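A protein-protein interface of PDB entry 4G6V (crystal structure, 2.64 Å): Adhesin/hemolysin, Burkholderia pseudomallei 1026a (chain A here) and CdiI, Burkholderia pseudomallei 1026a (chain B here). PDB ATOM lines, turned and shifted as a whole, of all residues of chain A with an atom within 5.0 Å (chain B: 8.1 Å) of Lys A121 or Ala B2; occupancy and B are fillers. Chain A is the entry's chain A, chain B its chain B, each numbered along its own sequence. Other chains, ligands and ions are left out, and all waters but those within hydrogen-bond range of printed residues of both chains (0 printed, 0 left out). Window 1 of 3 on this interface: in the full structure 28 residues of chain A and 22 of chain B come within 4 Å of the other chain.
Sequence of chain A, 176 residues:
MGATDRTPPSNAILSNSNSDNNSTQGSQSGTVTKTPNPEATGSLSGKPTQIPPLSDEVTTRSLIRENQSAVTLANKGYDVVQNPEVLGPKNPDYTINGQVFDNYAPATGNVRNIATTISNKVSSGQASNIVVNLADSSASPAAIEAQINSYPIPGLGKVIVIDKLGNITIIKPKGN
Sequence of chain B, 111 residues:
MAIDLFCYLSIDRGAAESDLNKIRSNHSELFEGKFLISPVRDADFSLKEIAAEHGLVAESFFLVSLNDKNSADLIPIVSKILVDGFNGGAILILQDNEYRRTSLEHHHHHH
OE1 of Glu A66 is in salt-bridge range of NZ of Lys B69 (3.0 Å). The side-chain carboxylate (OD2) of Asp A93 lies within hydrogen-bond range of the backbone NH (N) of Ala B2, 2.4 Å away. The side-chain carboxylate of Asp A93 lies within salt-bridge range of the side-chain amino group of Lys B69. The backbone carbonyl oxygen (O) of Asn A103 lies within hydrogen-bond range of the backbone NH (N) of Ala B2 (3.0 Å). The side-chain hydroxyl (OG1) of Thr A117 sits at hydrogen-bond distance from the side-chain amide nitrogen (ND2) of Asn B97, at 2.8 Å. The side-chain amino group of Lys A121 is in salt-bridge range of the side-chain carboxylate of Asp B4 (3.1 Å). The side-chain amino group (NZ) of Lys A121 is in salt-bridge range of the side-chain carboxylate (OD1) of Asp B96, at 2.9 Å.
The backbone NH (N) of Glu A66 sits close to the side-chain amide nitrogen (ND2) of Asn A103, at 3.4 Å. The side-chain carboxylate (OD2) of Asp A93 sits at hydrogen-bond distance from the backbone NH (N) of Asn A103. The backbone NH of Gly A125 lies within hydrogen-bond range of the backbone carbonyl oxygen of Asn A120, 3.4 Å away. The backbone NH of Gln A126 sits at hydrogen-bond distance from the backbone carbonyl oxygen of Lys A121. O of Lys A121 sits at hydrogen-bond distance from N of Ala A127 (3.2 Å). The backbone carbonyl oxygen (O) of Asp B4 is in hydrogen-bond range of the backbone NH (N) of Asp B96, 2.6 Å away.
Among the printed residues, merely in contact across the chains: Lys A121 with Ala B2, Asp A102 with Ala B2, Gly A125 with Leu B63, Thr A117 with Phe B6, Tyr A104 with Glu B98, Asn A120 with Phe B6, Thr A117 with Asp B96, Ser A124 with Leu B63 and Asn A120 with Leu B63.
Of the printed residues of chain B, Asn A103 touches Ala B2 (3.0 Å). Of chain B, only Ala B2 (3.5 Å), Asp B4 (3.1 Å) and Asp B96 (2.9 Å) come within 4 Å of Lys A121. Printed residues of chain B within 4 Å of Ser A124: Leu B63. Gly A125 touches just one residue of chain B: Leu B63. Leu B5 touches none of the printed residues of chain A. Phe B61 touches none of the printed residues of chain A. Of the printed residues of chain A, Asn B97 touches Thr A117 (2.8 Å). The nearest printed residue of chain A that does not touch Phe B6 is Lys A121 (4.4 Å).
Printed residues of chain B that touch a printed residue of chain A: Ala B2, Asp B4, Phe B6, Leu B63, Lys B69, Asp B96, Asn B97 and Glu B98. Hydrophobic or aromatic side chains of chain B that line the printed part of chain A: Ala B2, Phe B6 and Leu B63. Printed residues of chain A that touch a printed residue of chain B: Glu A66, Asp A93, Asp A102, Asn A103, Tyr A104, Thr A117, Asn A120, Lys A121, Ser A124 and Gly A125. Hydrophobic or aromatic side chains of chain A that line the printed part of chain B: Tyr A104. Among the printed residues, 16 pairs touch across the chains. Among the printed residues, Asp or Glu carboxylates within 4 Å of a Lys or Arg side-chain nitrogen of the other chain: Glu A66 with Lys B69 (3.0 Å), Asp A93 with Lys B69 (3.2 Å), Lys A121 with Asp B4 (3.1 Å) and Lys A121 with Asp B96 (2.9 Å).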
ATOM      1  N   GLU A  66      10.811 -16.065 -18.901  1.00  0.00           N
ATOM      2  CA  GLU A  66      11.082 -15.409 -20.177  1.00  0.00           C
ATOM      3  C   GLU A  66       9.864 -15.525 -21.111  1.00  0.00           C
ATOM      4  O   GLU A  66       9.406 -14.543 -21.698  1.00  0.00           O
ATOM      5  CB  GLU A  66      12.319 -16.014 -20.846  1.00  0.00           C
ATOM      6  CG  GLU A  66      12.649 -15.386 -22.185  1.00  0.00           C
ATOM      7  CD  GLU A  66      13.244 -16.379 -23.169  1.00  0.00           C
ATOM      8  OE1 GLU A  66      14.159 -17.116 -22.762  1.00  0.00           O
ATOM      9  OE2 GLU A  66      12.806 -16.413 -24.347  1.00  0.00           O
ATOM     10  N   ASP A  93      16.773 -12.568 -26.445  1.00  0.00           N
ATOM     11  CA  ASP A  93      15.500 -13.115 -26.016  1.00  0.00           C
ATOM     12  C   ASP A  93      14.332 -12.580 -26.845  1.00  0.00           C
ATOM     13  O   ASP A  93      13.551 -13.350 -27.416  1.00  0.00           O
ATOM     14  CB  ASP A  93      15.271 -12.789 -24.533  1.00  0.00           C
ATOM     15  CG  ASP A  93      16.143 -13.615 -23.607  1.00  0.00           C
ATOM     16  OD1 ASP A  93      16.683 -14.652 -24.061  1.00  0.00           O
ATOM     17  OD2 ASP A  93      16.275 -13.229 -22.421  1.00  0.00           O
ATOM     18  N   ASP A 102      16.600  -8.372 -23.448  1.00  0.00           N
ATOM     19  CA  ASP A 102      16.846  -9.642 -22.772  1.00  0.00           C
ATOM     20  C   ASP A 102      16.054  -9.721 -21.463  1.00  0.00           C
ATOM     21  O   ASP A 102      15.841  -8.699 -20.801  1.00  0.00           O
ATOM     22  CB  ASP A 102      18.340  -9.863 -22.521  1.00  0.00           C
ATOM     23  CG  ASP A 102      19.049 -10.511 -23.710  1.00  0.00           C
ATOM     24  OD1 ASP A 102      18.376 -10.840 -24.713  1.00  0.00           O
ATOM     25  OD2 ASP A 102      20.287 -10.697 -23.635  1.00  0.00           O
ATOM     26  N   ASN A 103      15.602 -10.928 -21.110  1.00  0.00           N
ATOM     27  CA  ASN A 103      14.874 -11.155 -19.856  1.00  0.00           C
ATOM     28  C   ASN A 103      15.824 -11.524 -18.735  1.00  0.00           C
ATOM     29  O   ASN A 103      16.765 -12.282 -18.939  1.00  0.00           O
ATOM     30  CB  ASN A 103      13.811 -12.266 -20.001  1.00  0.00           C
ATOM     31  CG  ASN A 103      12.926 -12.411 -18.748  1.00  0.00           C
ATOM     32  OD1 ASN A 103      12.182 -11.498 -18.405  1.00  0.00           O
ATOM     33  ND2 ASN A 103      13.017 -13.561 -18.056  1.00  0.00           N
ATOM     34  N   TYR A 104      15.573 -10.969 -17.555  1.00  0.00           N
ATOM     35  CA  TYR A 104      16.333 -11.299 -16.353  1.00  0.00           C
ATOM     36  C   TYR A 104      15.362 -11.426 -15.181  1.00  0.00           C
ATOM     37  O   TYR A 104      14.649 -10.476 -14.827  1.00  0.00           O
ATOM     38  CB  TYR A 104      17.422 -10.251 -16.095  1.00  0.00           C
ATOM     39  CG  TYR A 104      18.009 -10.233 -14.708  1.00  0.00           C
ATOM     40  CD1 TYR A 104      18.412 -11.406 -14.071  1.00  0.00           C
ATOM     41  CD2 TYR A 104      18.181  -9.036 -14.036  1.00  0.00           C
ATOM     42  CE1 TYR A 104      18.950 -11.373 -12.787  1.00  0.00           C
ATOM     43  CE2 TYR A 104      18.737  -8.992 -12.759  1.00  0.00           C
ATOM     44  CZ  TYR A 104      19.119 -10.154 -12.137  1.00  0.00           C
ATOM     45  OH  TYR A 104      19.680 -10.079 -10.866  1.00  0.00           O
ATOM     46  N   THR A 117      24.519  -7.422 -11.146  1.00  0.00           N
ATOM     47  CA  THR A 117      24.308  -8.513 -12.074  1.00  0.00           C
ATOM     48  C   THR A 117      24.009  -7.947 -13.442  1.00  0.00           C
ATOM     49  O   THR A 117      24.645  -8.309 -14.425  1.00  0.00           O
ATOM     50  CB  THR A 117      23.181  -9.462 -11.540  1.00  0.00           C
ATOM     51  OG1 THR A 117      23.634 -10.042 -10.311  1.00  0.00           O
ATOM     52  CG2 THR A 117      22.844 -10.576 -12.527  1.00  0.00           C
ATOM     53  N   ILE A 118      23.041  -7.044 -13.492  1.00  0.00           N
ATOM     54  CA  ILE A 118      22.718  -6.328 -14.708  1.00  0.00           C
ATOM     55  C   ILE A 118      23.964  -5.680 -15.304  1.00  0.00           C
ATOM     56  O   ILE A 118      24.289  -5.883 -16.486  1.00  0.00           O
ATOM     57  CB  ILE A 118      21.712  -5.209 -14.421  1.00  0.00           C
ATOM     58  CG1 ILE A 118      20.297  -5.780 -14.347  1.00  0.00           C
ATOM     59  CG2 ILE A 118      21.765  -4.156 -15.526  1.00  0.00           C
ATOM     60  CD1 ILE A 118      19.325  -4.889 -13.604  1.00  0.00           C
ATOM     61  N   SER A 119      24.643  -4.878 -14.488  1.00  0.00           N
ATOM     62  CA  SER A 119      25.867  -4.195 -14.915  1.00  0.00           C
ATOM     63  C   SER A 119      26.797  -5.147 -15.666  1.00  0.00           C
ATOM     64  O   SER A 119      27.221  -4.850 -16.794  1.00  0.00           O
ATOM     65  CB  SER A 119      26.588  -3.586 -13.712  1.00  0.00           C
ATOM     66  OG  SER A 119      27.623  -2.726 -14.138  1.00  0.00           O
ATOM     67  N   ASN A 120      27.078  -6.306 -15.055  1.00  0.00           N
ATOM     68  CA  ASN A 120      27.944  -7.303 -15.684  1.00  0.00           C
ATOM     69  C   ASN A 120      27.377  -8.043 -16.893  1.00  0.00           C
ATOM     70  O   ASN A 120      28.117  -8.376 -17.828  1.00  0.00           O
ATOM     71  CB  ASN A 120      28.520  -8.251 -14.654  1.00  0.00           C
ATOM     72  CG  ASN A 120      29.575  -7.578 -13.796  1.00  0.00           C
ATOM     73  OD1 ASN A 120      30.705  -7.340 -14.244  1.00  0.00           O
ATOM     74  ND2 ASN A 120      29.202  -7.216 -12.575  1.00  0.00           N
ATOM     75  N   LYS A 121      26.069  -8.277 -16.882  1.00  0.00           N
ATOM     76  CA  LYS A 121      25.396  -8.791 -18.057  1.00  0.00           C
ATOM     77  C   LYS A 121      25.631  -7.832 -19.215  1.00  0.00           C
ATOM     78  O   LYS A 121      25.797  -8.253 -20.353  1.00  0.00           O
ATOM     79  CB  LYS A 121      23.895  -8.956 -17.800  1.00  0.00           C
ATOM     80  CG  LYS A 121      23.508 -10.298 -17.249  1.00  0.00           C
ATOM     81  CD  LYS A 121      22.158 -10.229 -16.576  1.00  0.00           C
ATOM     82  CE  LYS A 121      21.703 -11.578 -16.014  1.00  0.00           C
ATOM     83  NZ  LYS A 121      21.602 -12.649 -17.054  1.00  0.00           N
ATOM     84  N   VAL A 122      25.642  -6.539 -18.915  1.00  0.00           N
ATOM     85  CA  VAL A 122      25.977  -5.532 -19.918  1.00  0.00           C
ATOM     86  C   VAL A 122      27.469  -5.541 -20.275  1.00  0.00           C
ATOM     87  O   VAL A 122      27.821  -5.784 -21.430  1.00  0.00           O
ATOM     88  CB  VAL A 122      25.526  -4.118 -19.495  1.00  0.00           C
ATOM     89  CG1 VAL A 122      26.073  -3.038 -20.476  1.00  0.00           C
ATOM     90  CG2 VAL A 122      23.997  -4.074 -19.386  1.00  0.00           C
ATOM     91  N   SER A 123      28.345  -5.299 -19.301  1.00  0.00           N
ATOM     92  CA  SER A 123      29.794  -5.237 -19.595  1.00  0.00           C
ATOM     93  C   SER A 123      30.406  -6.533 -20.155  1.00  0.00           C
ATOM     94  O   SER A 123      31.176  -6.488 -21.108  1.00  0.00           O
ATOM     95  CB  SER A 123      30.620  -4.717 -18.402  1.00  0.00           C
ATOM     96  OG  SER A 123      30.283  -5.339 -17.178  1.00  0.00           O
ATOM     97  N   SER A 124      30.070  -7.688 -19.586  1.00  0.00           N
ATOM     98  CA  SER A 124      30.664  -8.927 -20.100  1.00  0.00           C
ATOM     99  C   SER A 124      29.789  -9.649 -21.120  1.00  0.00           C
ATOM    100  O   SER A 124      30.300 -10.307 -22.033  1.00  0.00           O
ATOM    101  CB  SER A 124      31.061  -9.876 -18.968  1.00  0.00           C
ATOM    102  OG  SER A 124      32.326  -9.555 -18.439  1.00  0.00           O
ATOM    103  N   GLY A 125      28.475  -9.516 -20.965  1.00  0.00           N
ATOM    104  CA  GLY A 125      27.527 -10.206 -21.822  1.00  0.00           C
ATOM    105  C   GLY A 125      27.015  -9.408 -23.011  1.00  0.00           C
ATOM    106  O   GLY A 125      26.414  -9.984 -23.912  1.00  0.00           O
ATOM    107  N   GLN A 126      27.253  -8.093 -23.014  1.00  0.00           N
ATOM    108  CA  GLN A 126      26.879  -7.219 -24.126  1.00  0.00           C
ATOM    109  C   GLN A 126      25.368  -7.117 -24.270  1.00  0.00           C
ATOM    110  O   GLN A 126      24.817  -6.953 -25.378  1.00  0.00           O
ATOM    111  CB  GLN A 126      27.516  -7.683 -25.433  1.00  0.00           C
ATOM    112  CG  GLN A 126      29.012  -7.908 -25.331  1.00  0.00           C
ATOM    113  CD  GLN A 126      29.558  -8.620 -26.549  1.00  0.00           C
ATOM    114  OE1 GLN A 126      28.893  -9.493 -27.119  1.00  0.00           O
ATOM    115  NE2 GLN A 126      30.770  -8.244 -26.968  1.00  0.00           N
ATOM    116  N   ALA A 127      24.699  -7.241 -23.132  1.00  0.00           N
ATOM    117  CA  ALA A 127      23.292  -6.917 -23.065  1.00  0.00           C
ATOM    118  C   ALA A 127      23.176  -5.383 -23.063  1.00  0.00           C
ATOM    119  O   ALA A 127      24.120  -4.680 -22.687  1.00  0.00           O
ATOM    120  CB  ALA A 127      22.674  -7.518 -21.808  1.00  0.00           C
ATOM    121  N   ALA B   2      17.613 -14.510 -20.827  1.00  0.00           N
ATOM    122  CA  ALA B   2      19.032 -14.775 -21.055  1.00  0.00           C
ATOM    123  C   ALA B   2      19.651 -15.424 -19.826  1.00  0.00           C
ATOM    124  O   ALA B   2      19.496 -14.935 -18.702  1.00  0.00           O
ATOM    125  CB  ALA B   2      19.769 -13.489 -21.403  1.00  0.00           C
ATOM    126  N   ILE B   3      20.349 -16.532 -20.033  1.00  0.00           N
ATOM    127  CA  ILE B   3      20.974 -17.214 -18.899  1.00  0.00           C
ATOM    128  C   ILE B   3      22.496 -17.101 -18.900  1.00  0.00           C
ATOM    129  O   ILE B   3      23.162 -17.421 -19.887  1.00  0.00           O
ATOM    130  CB  ILE B   3      20.514 -18.677 -18.792  1.00  0.00           C
ATOM    131  CG1 ILE B   3      19.088 -18.719 -18.241  1.00  0.00           C
ATOM    132  CG2 ILE B   3      21.407 -19.440 -17.887  1.00  0.00           C
ATOM    133  CD1 ILE B   3      18.411 -20.075 -18.389  1.00  0.00           C
ATOM    134  N   ASP B   4      23.035 -16.626 -17.785  1.00  0.00           N
ATOM    135  CA  ASP B   4      24.463 -16.374 -17.698  1.00  0.00           C
ATOM    136  C   ASP B   4      25.071 -17.025 -16.461  1.00  0.00           C
ATOM    137  O   ASP B   4      24.566 -16.872 -15.351  1.00  0.00           O
ATOM    138  CB  ASP B   4      24.742 -14.861 -17.697  1.00  0.00           C
ATOM    139  CG  ASP B   4      24.434 -14.212 -19.039  1.00  0.00           C
ATOM    140  OD1 ASP B   4      24.766 -14.828 -20.078  1.00  0.00           O
ATOM    141  OD2 ASP B   4      23.857 -13.100 -19.063  1.00  0.00           O
ATOM    142  N   LEU B   5      26.162 -17.750 -16.667  1.00  0.00           N
ATOM    143  CA  LEU B   5      26.968 -18.262 -15.568  1.00  0.00           C
ATOM    144  C   LEU B   5      28.018 -17.214 -15.182  1.00  0.00           C
ATOM    145  O   LEU B   5      28.864 -16.823 -15.994  1.00  0.00           O
ATOM    146  CB  LEU B   5      27.601 -19.608 -15.954  1.00  0.00           C
ATOM    147  CG  LEU B   5      26.581 -20.688 -16.377  1.00  0.00           C
ATOM    148  CD1 LEU B   5      27.234 -21.995 -16.803  1.00  0.00           C
ATOM    149  CD2 LEU B   5      25.543 -20.951 -15.285  1.00  0.00           C
ATOM    150  N   PHE B   6      27.901 -16.724 -13.955  1.00  0.00           N
ATOM    151  CA  PHE B   6      28.868 -15.806 -13.389  1.00  0.00           C
ATOM    152  C   PHE B   6      29.982 -16.627 -12.771  1.00  0.00           C
ATOM    153  O   PHE B   6      29.744 -17.399 -11.861  1.00  0.00           O
ATOM    154  CB  PHE B   6      28.214 -14.957 -12.315  1.00  0.00           C
ATOM    155  CG  PHE B   6      27.524 -13.766 -12.850  1.00  0.00           C
ATOM    156  CD1 PHE B   6      27.883 -12.495 -12.443  1.00  0.00           C
ATOM    157  CD2 PHE B   6      26.530 -13.901 -13.800  1.00  0.00           C
ATOM    158  CE1 PHE B   6      27.240 -11.371 -12.976  1.00  0.00           C
ATOM    159  CE2 PHE B   6      25.876 -12.779 -14.330  1.00  0.00           C
ATOM    160  CZ  PHE B   6      26.237 -11.522 -13.919  1.00  0.00           C
ATOM    161  N   PHE B  61      37.158 -12.594 -13.112  1.00  0.00           N
ATOM    162  CA  PHE B  61      35.763 -12.920 -13.322  1.00  0.00           C
ATOM    163  C   PHE B  61      35.527 -13.056 -14.827  1.00  0.00           C
ATOM    164  O   PHE B  61      36.134 -12.347 -15.639  1.00  0.00           O
ATOM    165  CB  PHE B  61      34.882 -11.793 -12.782  1.00  0.00           C
ATOM    166  CG  PHE B  61      33.474 -11.871 -13.249  1.00  0.00           C
ATOM    167  CD1 PHE B  61      32.513 -12.488 -12.480  1.00  0.00           C
ATOM    168  CD2 PHE B  61      33.107 -11.352 -14.480  1.00  0.00           C
ATOM    169  CE1 PHE B  61      31.201 -12.572 -12.929  1.00  0.00           C
ATOM    170  CE2 PHE B  61      31.797 -11.432 -14.933  1.00  0.00           C
ATOM    171  CZ  PHE B  61      30.841 -12.038 -14.164  1.00  0.00           C
ATOM    172  N   LEU B  63      32.194 -14.374 -17.830  1.00  0.00           N
ATOM    173  CA  LEU B  63      30.809 -14.756 -17.994  1.00  0.00           C
ATOM    174  C   LEU B  63      30.681 -15.852 -19.048  1.00  0.00           C
ATOM    175  O   LEU B  63      31.444 -15.891 -20.018  1.00  0.00           O
ATOM    176  CB  LEU B  63      30.004 -13.525 -18.377  1.00  0.00           C
ATOM    177  CG  LEU B  63      28.514 -13.480 -18.053  1.00  0.00           C
ATOM    178  CD1 LEU B  63      28.312 -13.604 -16.557  1.00  0.00           C
ATOM    179  CD2 LEU B  63      27.889 -12.178 -18.587  1.00  0.00           C
ATOM    180  N   VAL B  64      29.735 -16.764 -18.826  1.00  0.00           N
ATOM    181  CA  VAL B  64      29.370 -17.777 -19.817  1.00  0.00           C
ATOM    182  C   VAL B  64      27.875 -17.651 -20.134  1.00  0.00           C
ATOM    183  O   VAL B  64      27.031 -17.882 -19.281  1.00  0.00           O
ATOM    184  CB  VAL B  64      29.675 -19.217 -19.336  1.00  0.00           C
ATOM    185  CG1 VAL B  64      29.383 -20.246 -20.423  1.00  0.00           C
ATOM    186  CG2 VAL B  64      31.111 -19.340 -18.936  1.00  0.00           C
ATOM    187  N   SER B  65      27.557 -17.271 -21.364  1.00  0.00           N
ATOM    188  CA  SER B  65      26.174 -17.081 -21.768  1.00  0.00           C
ATOM    189  C   SER B  65      25.626 -18.289 -22.481  1.00  0.00           C
ATOM    190  O   SER B  65      26.327 -18.928 -23.270  1.00  0.00           O
ATOM    191  CB  SER B  65      26.058 -15.872 -22.677  1.00  0.00           C
ATOM    192  OG  SER B  65      26.267 -14.687 -21.923  1.00  0.00           O
ATOM    193  N   LEU B  66      24.369 -18.599 -22.183  1.00  0.00           N
ATOM    194  CA  LEU B  66      23.655 -19.655 -22.871  1.00  0.00           C
ATOM    195  C   LEU B  66      23.149 -19.053 -24.186  1.00  0.00           C
ATOM    196  O   LEU B  66      22.195 -18.252 -24.215  1.00  0.00           O
ATOM    197  CB  LEU B  66      22.505 -20.192 -22.008  1.00  0.00           C
ATOM    198  CG  LEU B  66      21.581 -21.244 -22.640  1.00  0.00           C
ATOM    199  CD1 LEU B  66      22.298 -22.587 -22.827  1.00  0.00           C
ATOM    200  CD2 LEU B  66      20.258 -21.417 -21.849  1.00  0.00           C
ATOM    201  N   ASN B  67      23.815 -19.416 -25.277  1.00  0.00           N
ATOM    202  CA  ASN B  67      23.489 -18.841 -26.567  1.00  0.00           C
ATOM    203  C   ASN B  67      22.480 -19.659 -27.359  1.00  0.00           C
ATOM    204  O   ASN B  67      21.743 -19.123 -28.163  1.00  0.00           O
ATOM    205  CB  ASN B  67      24.752 -18.644 -27.393  1.00  0.00           C
ATOM    206  CG  ASN B  67      24.581 -17.589 -28.435  1.00  0.00           C
ATOM    207  OD1 ASN B  67      24.024 -16.521 -28.165  1.00  0.00           O
ATOM    208  ND2 ASN B  67      25.047 -17.874 -29.642  1.00  0.00           N
ATOM    209  N   LYS B  69      19.313 -21.874 -26.677  1.00  0.00           N
ATOM    210  CA  LYS B  69      18.329 -22.235 -25.660  1.00  0.00           C
ATOM    211  C   LYS B  69      18.127 -23.749 -25.559  1.00  0.00           C
ATOM    212  O   LYS B  69      17.933 -24.275 -24.477  1.00  0.00           O
ATOM    213  CB  LYS B  69      16.993 -21.536 -25.917  1.00  0.00           C
ATOM    214  CG  LYS B  69      17.031 -20.017 -25.760  1.00  0.00           C
ATOM    215  CD  LYS B  69      17.180 -19.600 -24.300  1.00  0.00           C
ATOM    216  CE  LYS B  69      16.949 -18.110 -24.139  1.00  0.00           C
ATOM    217  NZ  LYS B  69      15.965 -17.589 -25.168  1.00  0.00           N
ATOM    218  N   GLN B  95      24.839 -19.282 -11.392  1.00  0.00           N
ATOM    219  CA  GLN B  95      23.927 -19.071 -12.495  1.00  0.00           C
ATOM    220  C   GLN B  95      23.161 -17.781 -12.213  1.00  0.00           C
ATOM    221  O   GLN B  95      22.561 -17.621 -11.133  1.00  0.00           O
ATOM    222  CB  GLN B  95      22.981 -20.240 -12.628  1.00  0.00           C
ATOM    223  CG  GLN B  95      22.225 -20.233 -13.919  1.00  0.00           C
ATOM    224  CD  GLN B  95      21.675 -21.590 -14.275  1.00  0.00           C
ATOM    225  OE1 GLN B  95      22.248 -22.624 -13.917  1.00  0.00           O
ATOM    226  NE2 GLN B  95      20.563 -21.598 -14.991  1.00  0.00           N
ATOM    227  N   ASP B  96      23.220 -16.862 -13.180  1.00  0.00           N
ATOM    228  CA  ASP B  96      22.625 -15.532 -13.078  1.00  0.00           C
ATOM    229  C   ASP B  96      22.975 -14.851 -11.766  1.00  0.00           C
ATOM    230  O   ASP B  96      22.185 -14.071 -11.206  1.00  0.00           O
ATOM    231  CB  ASP B  96      21.105 -15.576 -13.325  1.00  0.00           C
ATOM    232  CG  ASP B  96      20.759 -15.723 -14.812  1.00  0.00           C
ATOM    233  OD1 ASP B  96      21.550 -15.224 -15.667  1.00  0.00           O
ATOM    234  OD2 ASP B  96      19.704 -16.336 -15.122  1.00  0.00           O
ATOM    235  N   ASN B  97      24.176 -15.165 -11.287  1.00  0.00           N
ATOM    236  CA  ASN B  97      24.752 -14.500 -10.132  1.00  0.00           C
ATOM    237  C   ASN B  97      23.909 -14.722  -8.884  1.00  0.00           C
ATOM    238  O   ASN B  97      23.941 -13.922  -7.953  1.00  0.00           O
ATOM    239  CB  ASN B  97      24.932 -12.999 -10.428  1.00  0.00           C
ATOM    240  CG  ASN B  97      26.170 -12.407  -9.758  1.00  0.00           C
ATOM    241  OD1 ASN B  97      27.128 -13.121  -9.430  1.00  0.00           O
ATOM    242  ND2 ASN B  97      26.146 -11.097  -9.541  1.00  0.00           N
ATOM    243  N   GLU B  98      23.163 -15.826  -8.877  1.00  0.00           N
ATOM    244  CA  GLU B  98      22.245 -16.162  -7.780  1.00  0.00           C
ATOM    245  C   GLU B  98      22.416 -17.576  -7.259  1.00  0.00           C
ATOM    246  O   GLU B  98      22.558 -17.779  -6.060  1.00  0.00           O
ATOM    247  CB  GLU B  98      20.783 -15.993  -8.209  1.00  0.00           C
ATOM    248  CG  GLU B  98      20.373 -14.554  -8.349  1.00  0.00           C
ATOM    249  CD  GLU B  98      18.945 -14.380  -8.798  1.00  0.00           C
ATOM    250  OE1 GLU B  98      18.621 -13.257  -9.225  1.00  0.00           O
ATOM    251  OE2 GLU B  98      18.153 -15.340  -8.734  1.00  0.00           O
